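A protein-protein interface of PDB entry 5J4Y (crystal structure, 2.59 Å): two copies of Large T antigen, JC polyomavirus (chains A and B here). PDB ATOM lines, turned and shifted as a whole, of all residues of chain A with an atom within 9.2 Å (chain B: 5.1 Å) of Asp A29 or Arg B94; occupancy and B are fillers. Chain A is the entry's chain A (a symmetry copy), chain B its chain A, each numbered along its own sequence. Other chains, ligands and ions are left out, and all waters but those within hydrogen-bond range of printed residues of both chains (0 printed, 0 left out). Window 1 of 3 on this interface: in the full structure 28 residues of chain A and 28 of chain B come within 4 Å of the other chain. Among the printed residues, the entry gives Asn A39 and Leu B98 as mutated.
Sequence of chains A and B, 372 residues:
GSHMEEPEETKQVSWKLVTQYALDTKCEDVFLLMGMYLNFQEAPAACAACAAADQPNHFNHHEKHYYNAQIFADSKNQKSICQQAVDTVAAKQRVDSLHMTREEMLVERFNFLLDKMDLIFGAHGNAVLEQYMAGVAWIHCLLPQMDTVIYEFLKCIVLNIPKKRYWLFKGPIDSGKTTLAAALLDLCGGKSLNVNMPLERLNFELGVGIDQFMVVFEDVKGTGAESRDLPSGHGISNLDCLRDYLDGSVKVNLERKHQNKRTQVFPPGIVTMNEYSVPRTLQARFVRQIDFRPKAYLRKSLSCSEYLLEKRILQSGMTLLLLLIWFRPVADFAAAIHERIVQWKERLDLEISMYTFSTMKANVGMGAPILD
The side-chain carboxylate of Asp A29 is in salt-bridge range of the guanidinium group of Arg B94.
NH2 of Arg B94 lies close to NE2 of Gln B259 (3.0 Å). The side-chain sulfur of Cys A27 lies within hydrogen-bond range of the backbone carbonyl oxygen of Asp A29 (3.3 Å). OD2 of Asp B211 lies within salt-bridge range of NH1 of Arg B94 (2.7 Å). OD1 of Asp A29 lies within hydrogen-bond range of N of Phe A31 (3.1 Å). The side-chain carboxylate (OD1) of Asp A29 is in hydrogen-bond range of the backbone NH (N) of Leu A32, 3.5 Å away. The backbone carbonyl oxygen (O) of Arg B94 sits at hydrogen-bond distance from the side-chain hydroxyl (OG) of Ser B97 (3.1 Å).
Among the printed residues, pairs that only touch across the chains: Phe A31 with Ala B91, Phe A31 with Gln B259, Leu A32 with Arg B94, Leu A32 with Val B95, Leu A32 with Leu B98, Met A34 with Ala B91, Gly A35 with Ala B91, Gly A35 with Val B95, Met A36 with Val B95 and Asn A39 with Val B95.
Of chain B, only Arg B94 (2.8 Å) comes within 4 Å of Asp A29. Of chain A, only Asp A29 (2.8 Å) and Leu A32 (3.7 Å) come within 4 Å of Arg B94. Val B95 touches just these residues of chain A: Leu A32 (3.9 Å), Gly A35 (3.5 Å), Met A36 (3.5 Å) and Asn A39 (3.7 Å). Printed residues of chain A within 4 Å of Leu B98: Leu A32 (3.8 Å). Printed residues of chain B within 4 Å of Phe A31: Ala B91 and Gln B259. Of the printed residues of chain A, Ala B91 touches Phe A31 (3.1 Å), Met A34 (3.9 Å) and Gly A35 (3.6 Å). Of the printed residues of chain B, Leu A32 touches Arg B94 (3.7 Å), Val B95 (3.9 Å) and Leu B98 (3.8 Å). Of the printed residues of chain B, Met A34 touches Ala B91 (3.9 Å). Ile B210 touches none of the printed residues of chain A. Val A18 touches none of the printed residues of chain B. The nearest residue of chain B that does not touch Asp A29 is Gln B259 (4.2 Å). The nearest residue of chain A that does not touch Arg B94 is Phe A31 (4.2 Å).
Printed residues of chain B that touch a printed residue of chain A: Ala B91, Arg B94, Val B95, Leu B98 and Gln B259. Along chain B the printed residues that touch a printed residue of chain A span positions 91 to 259. Hydrophobic or aromatic side chains of chain A within 4 Å of the printed part of chain B: Phe A31, Leu A32, Met A34 and Met A36. Among the printed residues, 11 pairs touch across the chains. Among the printed residues, Asp or Glu carboxylates within 4 Å of a Lys or Arg side-chain nitrogen of the other chain: Asp A29 with Arg B94.
1 position is printed for both chains.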
ATOM      1  N   VAL A  18       6.058 -26.000 -38.420  1.00  0.00           N
ATOM      2  CA  VAL A  18       6.540 -25.668 -37.071  1.00  0.00           C
ATOM      3  C   VAL A  18       5.550 -26.222 -35.999  1.00  0.00           C
ATOM      4  O   VAL A  18       5.971 -26.729 -34.947  1.00  0.00           O
ATOM      5  CB  VAL A  18       6.821 -24.151 -36.886  1.00  0.00           C
ATOM      6  CG1 VAL A  18       7.369 -23.851 -35.488  1.00  0.00           C
ATOM      7  CG2 VAL A  18       7.783 -23.635 -37.954  1.00  0.00           C
ATOM      8  N   TYR A  21       5.961 -29.991 -35.560  1.00  0.00           N
ATOM      9  CA  TYR A  21       7.099 -30.269 -34.691  1.00  0.00           C
ATOM     10  C   TYR A  21       6.736 -30.074 -33.184  1.00  0.00           C
ATOM     11  O   TYR A  21       7.050 -30.948 -32.362  1.00  0.00           O
ATOM     12  CB  TYR A  21       8.348 -29.470 -35.113  1.00  0.00           C
ATOM     13  CG  TYR A  21       9.482 -29.610 -34.120  1.00  0.00           C
ATOM     14  CD1 TYR A  21      10.168 -30.811 -33.979  1.00  0.00           C
ATOM     15  CD2 TYR A  21       9.813 -28.568 -33.265  1.00  0.00           C
ATOM     16  CE1 TYR A  21      11.152 -30.975 -33.011  1.00  0.00           C
ATOM     17  CE2 TYR A  21      10.781 -28.726 -32.276  1.00  0.00           C
ATOM     18  CZ  TYR A  21      11.450 -29.932 -32.150  1.00  0.00           C
ATOM     19  OH  TYR A  21      12.422 -30.085 -31.186  1.00  0.00           O
ATOM     20  N   ALA A  22       6.052 -28.957 -32.848  1.00  0.00           N
ATOM     21  CA  ALA A  22       5.576 -28.641 -31.496  1.00  0.00           C
ATOM     22  C   ALA A  22       4.603 -29.726 -31.002  1.00  0.00           C
ATOM     23  O   ALA A  22       4.737 -30.218 -29.866  1.00  0.00           O
ATOM     24  CB  ALA A  22       4.895 -27.283 -31.484  1.00  0.00           C
ATOM     25  N   THR A  25       6.494 -32.993 -30.171  1.00  0.00           N
ATOM     26  CA  THR A  25       7.307 -32.927 -28.952  1.00  0.00           C
ATOM     27  C   THR A  25       6.537 -32.481 -27.725  1.00  0.00           C
ATOM     28  O   THR A  25       7.148 -32.294 -26.672  1.00  0.00           O
ATOM     29  CB  THR A  25       8.536 -32.045 -29.199  1.00  0.00           C
ATOM     30  OG1 THR A  25       8.080 -30.751 -29.559  1.00  0.00           O
ATOM     31  CG2 THR A  25       9.417 -32.574 -30.308  1.00  0.00           C
ATOM     32  N   LYS A  26       5.200 -32.294 -27.856  1.00  0.00           N
ATOM     33  CA  LYS A  26       4.289 -31.805 -26.814  1.00  0.00           C
ATOM     34  C   LYS A  26       4.822 -30.454 -26.245  1.00  0.00           C
ATOM     35  O   LYS A  26       4.733 -30.205 -25.039  1.00  0.00           O
ATOM     36  CB  LYS A  26       4.068 -32.875 -25.724  1.00  0.00           C
ATOM     37  CG  LYS A  26       2.617 -33.096 -25.376  1.00  0.00           C
ATOM     38  CD  LYS A  26       2.399 -33.121 -23.861  1.00  0.00           C
ATOM     39  CE  LYS A  26       0.964 -33.452 -23.488  1.00  0.00           C
ATOM     40  NZ  LYS A  26       0.756 -33.530 -22.013  1.00  0.00           N
ATOM     41  N   CYS A  27       5.362 -29.584 -27.141  1.00  0.00           N
ATOM     42  CA  CYS A  27       5.967 -28.300 -26.766  1.00  0.00           C
ATOM     43  C   CYS A  27       4.979 -27.240 -26.296  1.00  0.00           C
ATOM     44  O   CYS A  27       4.139 -26.797 -27.068  1.00  0.00           O
ATOM     45  CB  CYS A  27       6.863 -27.750 -27.870  1.00  0.00           C
ATOM     46  SG  CYS A  27       8.008 -26.467 -27.304  1.00  0.00           S
ATOM     47  N   GLU A  28       5.157 -26.786 -25.038  1.00  0.00           N
ATOM     48  CA  GLU A  28       4.352 -25.766 -24.368  1.00  0.00           C
ATOM     49  C   GLU A  28       5.120 -24.456 -24.162  1.00  0.00           C
ATOM     50  O   GLU A  28       4.559 -23.499 -23.617  1.00  0.00           O
ATOM     51  CB  GLU A  28       3.882 -26.298 -23.017  1.00  0.00           C
ATOM     52  CG  GLU A  28       2.919 -27.463 -23.122  1.00  0.00           C
ATOM     53  CD  GLU A  28       3.025 -28.457 -21.986  1.00  0.00           C
ATOM     54  OE1 GLU A  28       3.123 -28.013 -20.819  1.00  0.00           O
ATOM     55  OE2 GLU A  28       2.999 -29.681 -22.260  1.00  0.00           O
ATOM     56  N   ASP A  29       6.403 -24.409 -24.593  1.00  0.00           N
ATOM     57  CA  ASP A  29       7.296 -23.252 -24.443  1.00  0.00           C
ATOM     58  C   ASP A  29       7.651 -22.621 -25.804  1.00  0.00           C
ATOM     59  O   ASP A  29       8.267 -23.275 -26.639  1.00  0.00           O
ATOM     60  CB  ASP A  29       8.560 -23.697 -23.676  1.00  0.00           C
ATOM     61  CG  ASP A  29       9.548 -22.629 -23.233  1.00  0.00           C
ATOM     62  OD1 ASP A  29       9.350 -21.425 -23.592  1.00  0.00           O
ATOM     63  OD2 ASP A  29      10.505 -22.981 -22.513  1.00  0.00           O
ATOM     64  N   VAL A  30       7.285 -21.342 -25.998  1.00  0.00           N
ATOM     65  CA  VAL A  30       7.553 -20.540 -27.210  1.00  0.00           C
ATOM     66  C   VAL A  30       9.069 -20.318 -27.420  1.00  0.00           C
ATOM     67  O   VAL A  30       9.551 -20.408 -28.554  1.00  0.00           O
ATOM     68  CB  VAL A  30       6.745 -19.196 -27.205  1.00  0.00           C
ATOM     69  CG1 VAL A  30       7.282 -18.189 -28.221  1.00  0.00           C
ATOM     70  CG2 VAL A  30       5.268 -19.461 -27.470  1.00  0.00           C
ATOM     71  N   PHE A  31       9.803 -20.030 -26.334  1.00  0.00           N
ATOM     72  CA  PHE A  31      11.231 -19.810 -26.421  1.00  0.00           C
ATOM     73  C   PHE A  31      11.984 -21.079 -26.722  1.00  0.00           C
ATOM     74  O   PHE A  31      12.838 -21.058 -27.599  1.00  0.00           O
ATOM     75  CB  PHE A  31      11.767 -19.084 -25.190  1.00  0.00           C
ATOM     76  CG  PHE A  31      11.320 -17.639 -25.184  1.00  0.00           C
ATOM     77  CD1 PHE A  31      10.211 -17.242 -24.447  1.00  0.00           C
ATOM     78  CD2 PHE A  31      11.942 -16.698 -26.000  1.00  0.00           C
ATOM     79  CE1 PHE A  31       9.765 -15.921 -24.485  1.00  0.00           C
ATOM     80  CE2 PHE A  31      11.500 -15.379 -26.032  1.00  0.00           C
ATOM     81  CZ  PHE A  31      10.422 -14.994 -25.266  1.00  0.00           C
ATOM     82  N   LEU A  32      11.613 -22.206 -26.100  1.00  0.00           N
ATOM     83  CA  LEU A  32      12.270 -23.474 -26.407  1.00  0.00           C
ATOM     84  C   LEU A  32      11.935 -23.935 -27.827  1.00  0.00           C
ATOM     85  O   LEU A  32      12.780 -24.529 -28.478  1.00  0.00           O
ATOM     86  CB  LEU A  32      11.896 -24.531 -25.374  1.00  0.00           C
ATOM     87  CG  LEU A  32      12.509 -25.920 -25.537  1.00  0.00           C
ATOM     88  CD1 LEU A  32      13.975 -25.921 -25.196  1.00  0.00           C
ATOM     89  CD2 LEU A  32      11.771 -26.904 -24.694  1.00  0.00           C
ATOM     90  N   LEU A  33      10.739 -23.626 -28.322  1.00  0.00           N
ATOM     91  CA  LEU A  33      10.371 -23.987 -29.683  1.00  0.00           C
ATOM     92  C   LEU A  33      11.183 -23.206 -30.722  1.00  0.00           C
ATOM     93  O   LEU A  33      11.651 -23.800 -31.705  1.00  0.00           O
ATOM     94  CB  LEU A  33       8.872 -23.826 -29.918  1.00  0.00           C
ATOM     95  CG  LEU A  33       8.351 -24.242 -31.291  1.00  0.00           C
ATOM     96  CD1 LEU A  33       8.741 -25.659 -31.635  1.00  0.00           C
ATOM     97  CD2 LEU A  33       6.856 -24.074 -31.352  1.00  0.00           C
ATOM     98  N   MET A  34      11.373 -21.894 -30.478  1.00  0.00           N
ATOM     99  CA  MET A  34      12.172 -20.991 -31.298  1.00  0.00           C
ATOM    100  C   MET A  34      13.592 -21.526 -31.376  1.00  0.00           C
ATOM    101  O   MET A  34      14.120 -21.705 -32.475  1.00  0.00           O
ATOM    102  CB  MET A  34      12.203 -19.631 -30.622  1.00  0.00           C
ATOM    103  CG  MET A  34      11.755 -18.500 -31.487  1.00  0.00           C
ATOM    104  SD  MET A  34      11.581 -17.040 -30.450  1.00  0.00           S
ATOM    105  CE  MET A  34      12.566 -15.852 -31.402  1.00  0.00           C
ATOM    106  N   GLY A  35      14.170 -21.828 -30.204  1.00  0.00           N
ATOM    107  CA  GLY A  35      15.515 -22.370 -30.046  1.00  0.00           C
ATOM    108  C   GLY A  35      15.689 -23.699 -30.748  1.00  0.00           C
ATOM    109  O   GLY A  35      16.580 -23.827 -31.592  1.00  0.00           O
ATOM    110  N   MET A  36      14.813 -24.693 -30.428  1.00  0.00           N
ATOM    111  CA  MET A  36      14.809 -26.028 -31.062  1.00  0.00           C
ATOM    112  C   MET A  36      14.697 -25.941 -32.589  1.00  0.00           C
ATOM    113  O   MET A  36      15.538 -26.513 -33.278  1.00  0.00           O
ATOM    114  CB  MET A  36      13.701 -26.938 -30.496  1.00  0.00           C
ATOM    115  CG  MET A  36      13.949 -27.371 -29.046  1.00  0.00           C
ATOM    116  SD  MET A  36      15.567 -28.150 -28.754  1.00  0.00           S
ATOM    117  CE  MET A  36      15.286 -29.787 -29.452  1.00  0.00           C
ATOM    118  N   TYR A  37      13.723 -25.152 -33.109  1.00  0.00           N
ATOM    119  CA  TYR A  37      13.533 -24.994 -34.552  1.00  0.00           C
ATOM    120  C   TYR A  37      14.719 -24.303 -35.265  1.00  0.00           C
ATOM    121  O   TYR A  37      15.045 -24.677 -36.390  1.00  0.00           O
ATOM    122  CB  TYR A  37      12.191 -24.329 -34.904  1.00  0.00           C
ATOM    123  CG  TYR A  37      11.584 -24.953 -36.145  1.00  0.00           C
ATOM    124  CD1 TYR A  37      11.757 -24.368 -37.401  1.00  0.00           C
ATOM    125  CD2 TYR A  37      10.864 -26.150 -36.072  1.00  0.00           C
ATOM    126  CE1 TYR A  37      11.193 -24.933 -38.548  1.00  0.00           C
ATOM    127  CE2 TYR A  37      10.295 -26.725 -37.214  1.00  0.00           C
ATOM    128  CZ  TYR A  37      10.474 -26.117 -38.451  1.00  0.00           C
ATOM    129  OH  TYR A  37       9.943 -26.673 -39.583  1.00  0.00           O
ATOM    130  N   ASN A  39      17.993 -24.585 -34.420  1.00  0.00           N
ATOM    131  CA  ASN A  39      19.119 -25.533 -34.477  1.00  0.00           C
ATOM    132  C   ASN A  39      19.062 -26.512 -35.657  1.00  0.00           C
ATOM    133  O   ASN A  39      20.054 -27.181 -35.938  1.00  0.00           O
ATOM    134  CB  ASN A  39      19.273 -26.282 -33.152  1.00  0.00           C
ATOM    135  CG  ASN A  39      19.919 -25.478 -32.047  1.00  0.00           C
ATOM    136  OD1 ASN A  39      20.299 -24.311 -32.207  1.00  0.00           O
ATOM    137  ND2 ASN A  39      20.055 -26.088 -30.890  1.00  0.00           N
ATOM    138  N   LYS A  79       8.571 -15.245 -33.267  1.00  0.00           N
ATOM    139  CA  LYS A  79       7.799 -15.402 -32.023  1.00  0.00           C
ATOM    140  C   LYS A  79       6.317 -15.703 -32.271  1.00  0.00           C
ATOM    141  O   LYS A  79       5.738 -16.497 -31.526  1.00  0.00           O
ATOM    142  CB  LYS A  79       7.986 -14.190 -31.095  1.00  0.00           C
ATOM    143  CG  LYS A  79       7.608 -14.420 -29.629  1.00  0.00           C
ATOM    144  CD  LYS A  79       7.674 -13.107 -28.863  1.00  0.00           C
ATOM    145  CE  LYS A  79       7.638 -13.253 -27.360  1.00  0.00           C
ATOM    146  NZ  LYS A  79       8.195 -12.034 -26.686  1.00  0.00           N
ATOM    147  N   CYS A  82       5.822 -19.325 -33.494  1.00  0.00           N
ATOM    148  CA  CYS A  82       5.916 -20.221 -32.341  1.00  0.00           C
ATOM    149  C   CYS A  82       4.745 -20.098 -31.348  1.00  0.00           C
ATOM    150  O   CYS A  82       4.394 -21.099 -30.706  1.00  0.00           O
ATOM    151  CB  CYS A  82       7.267 -20.052 -31.663  1.00  0.00           C
ATOM    152  SG  CYS A  82       8.649 -20.408 -32.771  1.00  0.00           S
ATOM    153  N   GLN A  83       4.125 -18.902 -31.257  1.00  0.00           N
ATOM    154  CA  GLN A  83       2.930 -18.668 -30.443  1.00  0.00           C
ATOM    155  C   GLN A  83       1.735 -19.524 -30.968  1.00  0.00           C
ATOM    156  O   GLN A  83       1.115 -20.259 -30.185  1.00  0.00           O
ATOM    157  CB  GLN A  83       2.576 -17.183 -30.389  1.00  0.00           C
ATOM    158  CG  GLN A  83       1.632 -16.845 -29.241  1.00  0.00           C
ATOM    159  CD  GLN A  83       2.031 -17.487 -27.915  1.00  0.00           C
ATOM    160  OE1 GLN A  83       3.055 -17.154 -27.297  1.00  0.00           O
ATOM    161  NE2 GLN A  83       1.231 -18.438 -27.459  1.00  0.00           N
ATOM    162  N   ALA A  85       1.986 -22.227 -32.830  1.00  0.00           N
ATOM    163  CA  ALA A  85       2.362 -23.633 -32.640  1.00  0.00           C
ATOM    164  C   ALA A  85       2.066 -24.098 -31.210  1.00  0.00           C
ATOM    165  O   ALA A  85       1.412 -25.114 -31.023  1.00  0.00           O
ATOM    166  CB  ALA A  85       3.823 -23.833 -32.969  1.00  0.00           C
ATOM    167  N   VAL A  86       2.460 -23.310 -30.224  1.00  0.00           N
ATOM    168  CA  VAL A  86       2.249 -23.568 -28.801  1.00  0.00           C
ATOM    169  C   VAL A  86       0.751 -23.515 -28.463  1.00  0.00           C
ATOM    170  O   VAL A  86       0.285 -24.400 -27.750  1.00  0.00           O
ATOM    171  CB  VAL A  86       3.155 -22.649 -27.931  1.00  0.00           C
ATOM    172  CG1 VAL A  86       2.674 -22.549 -26.481  1.00  0.00           C
ATOM    173  CG2 VAL A  86       4.602 -23.150 -27.985  1.00  0.00           C
ATOM    174  N   ASP A  87      -0.004 -22.566 -29.048  1.00  0.00           N
ATOM    175  CA  ASP A  87      -1.463 -22.468 -28.902  1.00  0.00           C
ATOM    176  C   ASP A  87      -2.194 -23.703 -29.444  1.00  0.00           C
ATOM    177  O   ASP A  87      -3.135 -24.157 -28.808  1.00  0.00           O
ATOM    178  CB  ASP A  87      -2.021 -21.188 -29.572  1.00  0.00           C
ATOM    179  CG  ASP A  87      -1.570 -19.868 -28.949  1.00  0.00           C
ATOM    180  OD1 ASP A  87      -1.227 -19.858 -27.739  1.00  0.00           O
ATOM    181  OD2 ASP A  87      -1.512 -18.856 -29.684  1.00  0.00           O
ATOM    182  N   VAL A  89      -0.915 -26.705 -29.610  1.00  0.00           N
ATOM    183  CA  VAL A  89      -0.615 -27.736 -28.615  1.00  0.00           C
ATOM    184  C   VAL A  89      -1.609 -27.565 -27.433  1.00  0.00           C
ATOM    185  O   VAL A  89      -2.196 -28.557 -26.994  1.00  0.00           O
ATOM    186  CB  VAL A  89       0.885 -27.767 -28.145  1.00  0.00           C
ATOM    187  CG1 VAL A  89       1.130 -28.889 -27.138  1.00  0.00           C
ATOM    188  CG2 VAL A  89       1.838 -27.912 -29.327  1.00  0.00           C
ATOM    189  N   ALA A  90      -1.816 -26.323 -26.944  1.00  0.00           N
ATOM    190  CA  ALA A  90      -2.792 -26.082 -25.857  1.00  0.00           C
ATOM    191  C   ALA A  90      -4.246 -26.487 -26.304  1.00  0.00           C
ATOM    192  O   ALA A  90      -4.985 -27.112 -25.534  1.00  0.00           O
ATOM    193  CB  ALA A  90      -2.747 -24.627 -25.400  1.00  0.00           C
ATOM    194  N   ALA B  90      17.486 -15.642 -25.553  1.00  0.00           N
ATOM    195  CA  ALA B  90      16.733 -16.324 -24.475  1.00  0.00           C
ATOM    196  C   ALA B  90      16.375 -17.801 -24.883  1.00  0.00           C
ATOM    197  O   ALA B  90      16.506 -18.723 -24.068  1.00  0.00           O
ATOM    198  CB  ALA B  90      15.476 -15.538 -24.110  1.00  0.00           C
ATOM    199  N   ALA B  91      15.978 -17.999 -26.155  1.00  0.00           N
ATOM    200  CA  ALA B  91      15.662 -19.285 -26.774  1.00  0.00           C
ATOM    201  C   ALA B  91      16.899 -20.239 -26.752  1.00  0.00           C
ATOM    202  O   ALA B  91      16.735 -21.428 -26.450  1.00  0.00           O
ATOM    203  CB  ALA B  91      15.176 -19.059 -28.199  1.00  0.00           C
ATOM    204  N   LYS B  92      18.128 -19.705 -27.014  1.00  0.00           N
ATOM    205  CA  LYS B  92      19.399 -20.450 -26.950  1.00  0.00           C
ATOM    206  C   LYS B  92      19.621 -21.004 -25.542  1.00  0.00           C
ATOM    207  O   LYS B  92      19.833 -22.202 -25.382  1.00  0.00           O
ATOM    208  CB  LYS B  92      20.587 -19.553 -27.360  1.00  0.00           C
ATOM    209  CG  LYS B  92      21.757 -20.311 -27.963  1.00  0.00           C
ATOM    210  CD  LYS B  92      22.942 -20.371 -27.026  1.00  0.00           C
ATOM    211  CE  LYS B  92      24.153 -20.976 -27.686  1.00  0.00           C
ATOM    212  NZ  LYS B  92      25.186 -21.345 -26.688  1.00  0.00           N
ATOM    213  N   GLN B  93      19.492 -20.148 -24.524  1.00  0.00           N
ATOM    214  CA  GLN B  93      19.602 -20.538 -23.114  1.00  0.00           C
ATOM    215  C   GLN B  93      18.616 -21.646 -22.708  1.00  0.00           C
ATOM    216  O   GLN B  93      18.995 -22.527 -21.936  1.00  0.00           O
ATOM    217  CB  GLN B  93      19.492 -19.321 -22.172  1.00  0.00           C
ATOM    218  CG  GLN B  93      20.446 -18.141 -22.488  1.00  0.00           C
ATOM    219  CD  GLN B  93      21.862 -18.544 -22.854  1.00  0.00           C
ATOM    220  OE1 GLN B  93      22.524 -19.312 -22.135  1.00  0.00           O
ATOM    221  NE2 GLN B  93      22.364 -18.022 -23.981  1.00  0.00           N
ATOM    222  N   ARG B  94      17.363 -21.627 -23.241  1.00  0.00           N
ATOM    223  CA  ARG B  94      16.376 -22.678 -22.929  1.00  0.00           C
ATOM    224  C   ARG B  94      16.805 -24.028 -23.458  1.00  0.00           C
ATOM    225  O   ARG B  94      16.668 -25.033 -22.755  1.00  0.00           O
ATOM    226  CB  ARG B  94      14.967 -22.356 -23.452  1.00  0.00           C
ATOM    227  CG  ARG B  94      14.204 -21.368 -22.617  1.00  0.00           C
ATOM    228  CD  ARG B  94      13.588 -21.939 -21.356  1.00  0.00           C
ATOM    229  NE  ARG B  94      12.280 -21.331 -21.099  1.00  0.00           N
ATOM    230  CZ  ARG B  94      12.082 -20.106 -20.618  1.00  0.00           C
ATOM    231  NH1 ARG B  94      13.113 -19.333 -20.311  1.00  0.00           N
ATOM    232  NH2 ARG B  94      10.853 -19.648 -20.438  1.00  0.00           N
ATOM    233  N   VAL B  95      17.313 -24.051 -24.700  1.00  0.00           N
ATOM    234  CA  VAL B  95      17.779 -25.280 -25.348  1.00  0.00           C
ATOM    235  C   VAL B  95      18.999 -25.780 -24.603  1.00  0.00           C
ATOM    236  O   VAL B  95      19.066 -26.961 -24.280  1.00  0.00           O
ATOM    237  CB  VAL B  95      18.043 -25.097 -26.868  1.00  0.00           C
ATOM    238  CG1 VAL B  95      18.595 -26.379 -27.490  1.00  0.00           C
ATOM    239  CG2 VAL B  95      16.773 -24.663 -27.581  1.00  0.00           C
ATOM    240  N   ASP B  96      19.933 -24.854 -24.294  1.00  0.00           N
ATOM    241  CA  ASP B  96      21.151 -25.143 -23.552  1.00  0.00           C
ATOM    242  C   ASP B  96      20.810 -25.745 -22.201  1.00  0.00           C
ATOM    243  O   ASP B  96      21.185 -26.891 -21.971  1.00  0.00           O
ATOM    244  CB  ASP B  96      22.053 -23.900 -23.441  1.00  0.00           C
ATOM    245  CG  ASP B  96      22.760 -23.495 -24.731  1.00  0.00           C
ATOM    246  OD1 ASP B  96      22.407 -24.035 -25.809  1.00  0.00           O
ATOM    247  OD2 ASP B  96      23.687 -22.665 -24.659  1.00  0.00           O
ATOM    248  N   SER B  97      19.959 -25.082 -21.396  1.00  0.00           N
ATOM    249  CA  SER B  97      19.568 -25.604 -20.081  1.00  0.00           C
ATOM    250  C   SER B  97      19.025 -27.072 -20.116  1.00  0.00           C
ATOM    251  O   SER B  97      19.190 -27.789 -19.123  1.00  0.00           O
ATOM    252  CB  SER B  97      18.609 -24.658 -19.355  1.00  0.00           C
ATOM    253  OG  SER B  97      17.251 -24.856 -19.707  1.00  0.00           O
ATOM    254  N   LEU B  98      18.489 -27.534 -21.272  1.00  0.00           N
ATOM    255  CA  LEU B  98      17.960 -28.902 -21.420  1.00  0.00           C
ATOM    256  C   LEU B  98      18.833 -29.885 -22.241  1.00  0.00           C
ATOM    257  O   LEU B  98      18.678 -31.100 -22.071  1.00  0.00           O
ATOM    258  CB  LEU B  98      16.530 -28.877 -22.000  1.00  0.00           C
ATOM    259  CG  LEU B  98      15.488 -28.077 -21.203  1.00  0.00           C
ATOM    260  CD1 LEU B  98      14.237 -27.886 -21.998  1.00  0.00           C
ATOM    261  CD2 LEU B  98      15.176 -28.724 -19.843  1.00  0.00           C
ATOM    262  N   ILE B 210      15.292 -18.269 -13.353  1.00  0.00           N
ATOM    263  CA  ILE B 210      15.011 -18.965 -14.614  1.00  0.00           C
ATOM    264  C   ILE B 210      16.262 -18.982 -15.524  1.00  0.00           C
ATOM    265  O   ILE B 210      16.865 -17.929 -15.759  1.00  0.00           O
ATOM    266  CB  ILE B 210      13.732 -18.384 -15.289  1.00  0.00           C
ATOM    267  CG1 ILE B 210      12.474 -18.927 -14.579  1.00  0.00           C
ATOM    268  CG2 ILE B 210      13.672 -18.670 -16.804  1.00  0.00           C
ATOM    269  CD1 ILE B 210      11.215 -18.073 -14.714  1.00  0.00           C
ATOM    270  N   ASP B 211      16.658 -20.200 -15.982  1.00  0.00           N
ATOM    271  CA  ASP B 211      17.805 -20.516 -16.861  1.00  0.00           C
ATOM    272  C   ASP B 211      19.177 -20.163 -16.264  1.00  0.00           C
ATOM    273  O   ASP B 211      20.194 -20.235 -16.965  1.00  0.00           O
ATOM    274  CB  ASP B 211      17.655 -19.887 -18.267  1.00  0.00           C
ATOM    275  CG  ASP B 211      16.403 -20.293 -19.017  1.00  0.00           C
ATOM    276  OD1 ASP B 211      16.135 -21.505 -19.115  1.00  0.00           O
ATOM    277  OD2 ASP B 211      15.730 -19.404 -19.562  1.00  0.00           O
ATOM    278  N   GLN B 259       4.973 -13.946 -19.138  1.00  0.00           N
ATOM    279  CA  GLN B 259       5.538 -15.255 -19.468  1.00  0.00           C
ATOM    280  C   GLN B 259       4.803 -16.369 -18.722  1.00  0.00           C
ATOM    281  O   GLN B 259       4.456 -16.203 -17.547  1.00  0.00           O
ATOM    282  CB  GLN B 259       7.054 -15.270 -19.112  1.00  0.00           C
ATOM    283  CG  GLN B 259       7.826 -16.584 -19.376  1.00  0.00           C
ATOM    284  CD  GLN B 259       8.008 -16.945 -20.838  1.00  0.00           C
ATOM    285  OE1 GLN B 259       7.904 -16.109 -21.748  1.00  0.00           O
ATOM    286  NE2 GLN B 259       8.296 -18.211 -21.094  1.00  0.00           N
ATOM    287  N   ARG B 262       7.652 -20.968 -15.796  1.00  0.00           N
ATOM    288  CA  ARG B 262       8.675 -21.954 -16.148  1.00  0.00           C
ATOM    289  C   ARG B 262       8.846 -23.057 -15.117  1.00  0.00           C
ATOM    290  O   ARG B 262       8.933 -22.778 -13.924  1.00  0.00           O
ATOM    291  CB  ARG B 262      10.030 -21.264 -16.402  1.00  0.00           C
ATOM    292  CG  ARG B 262      10.701 -21.660 -17.711  1.00  0.00           C
ATOM    293  CD  ARG B 262      11.445 -22.984 -17.650  1.00  0.00           C
ATOM    294  NE  ARG B 262      12.889 -22.808 -17.490  1.00  0.00           N
ATOM    295  CZ  ARG B 262      13.791 -23.739 -17.791  1.00  0.00           C
ATOM    296  NH1 ARG B 262      13.406 -24.916 -18.273  1.00  0.00           N
ATOM    297  NH2 ARG B 262      15.081 -23.505 -17.603  1.00  0.00           N
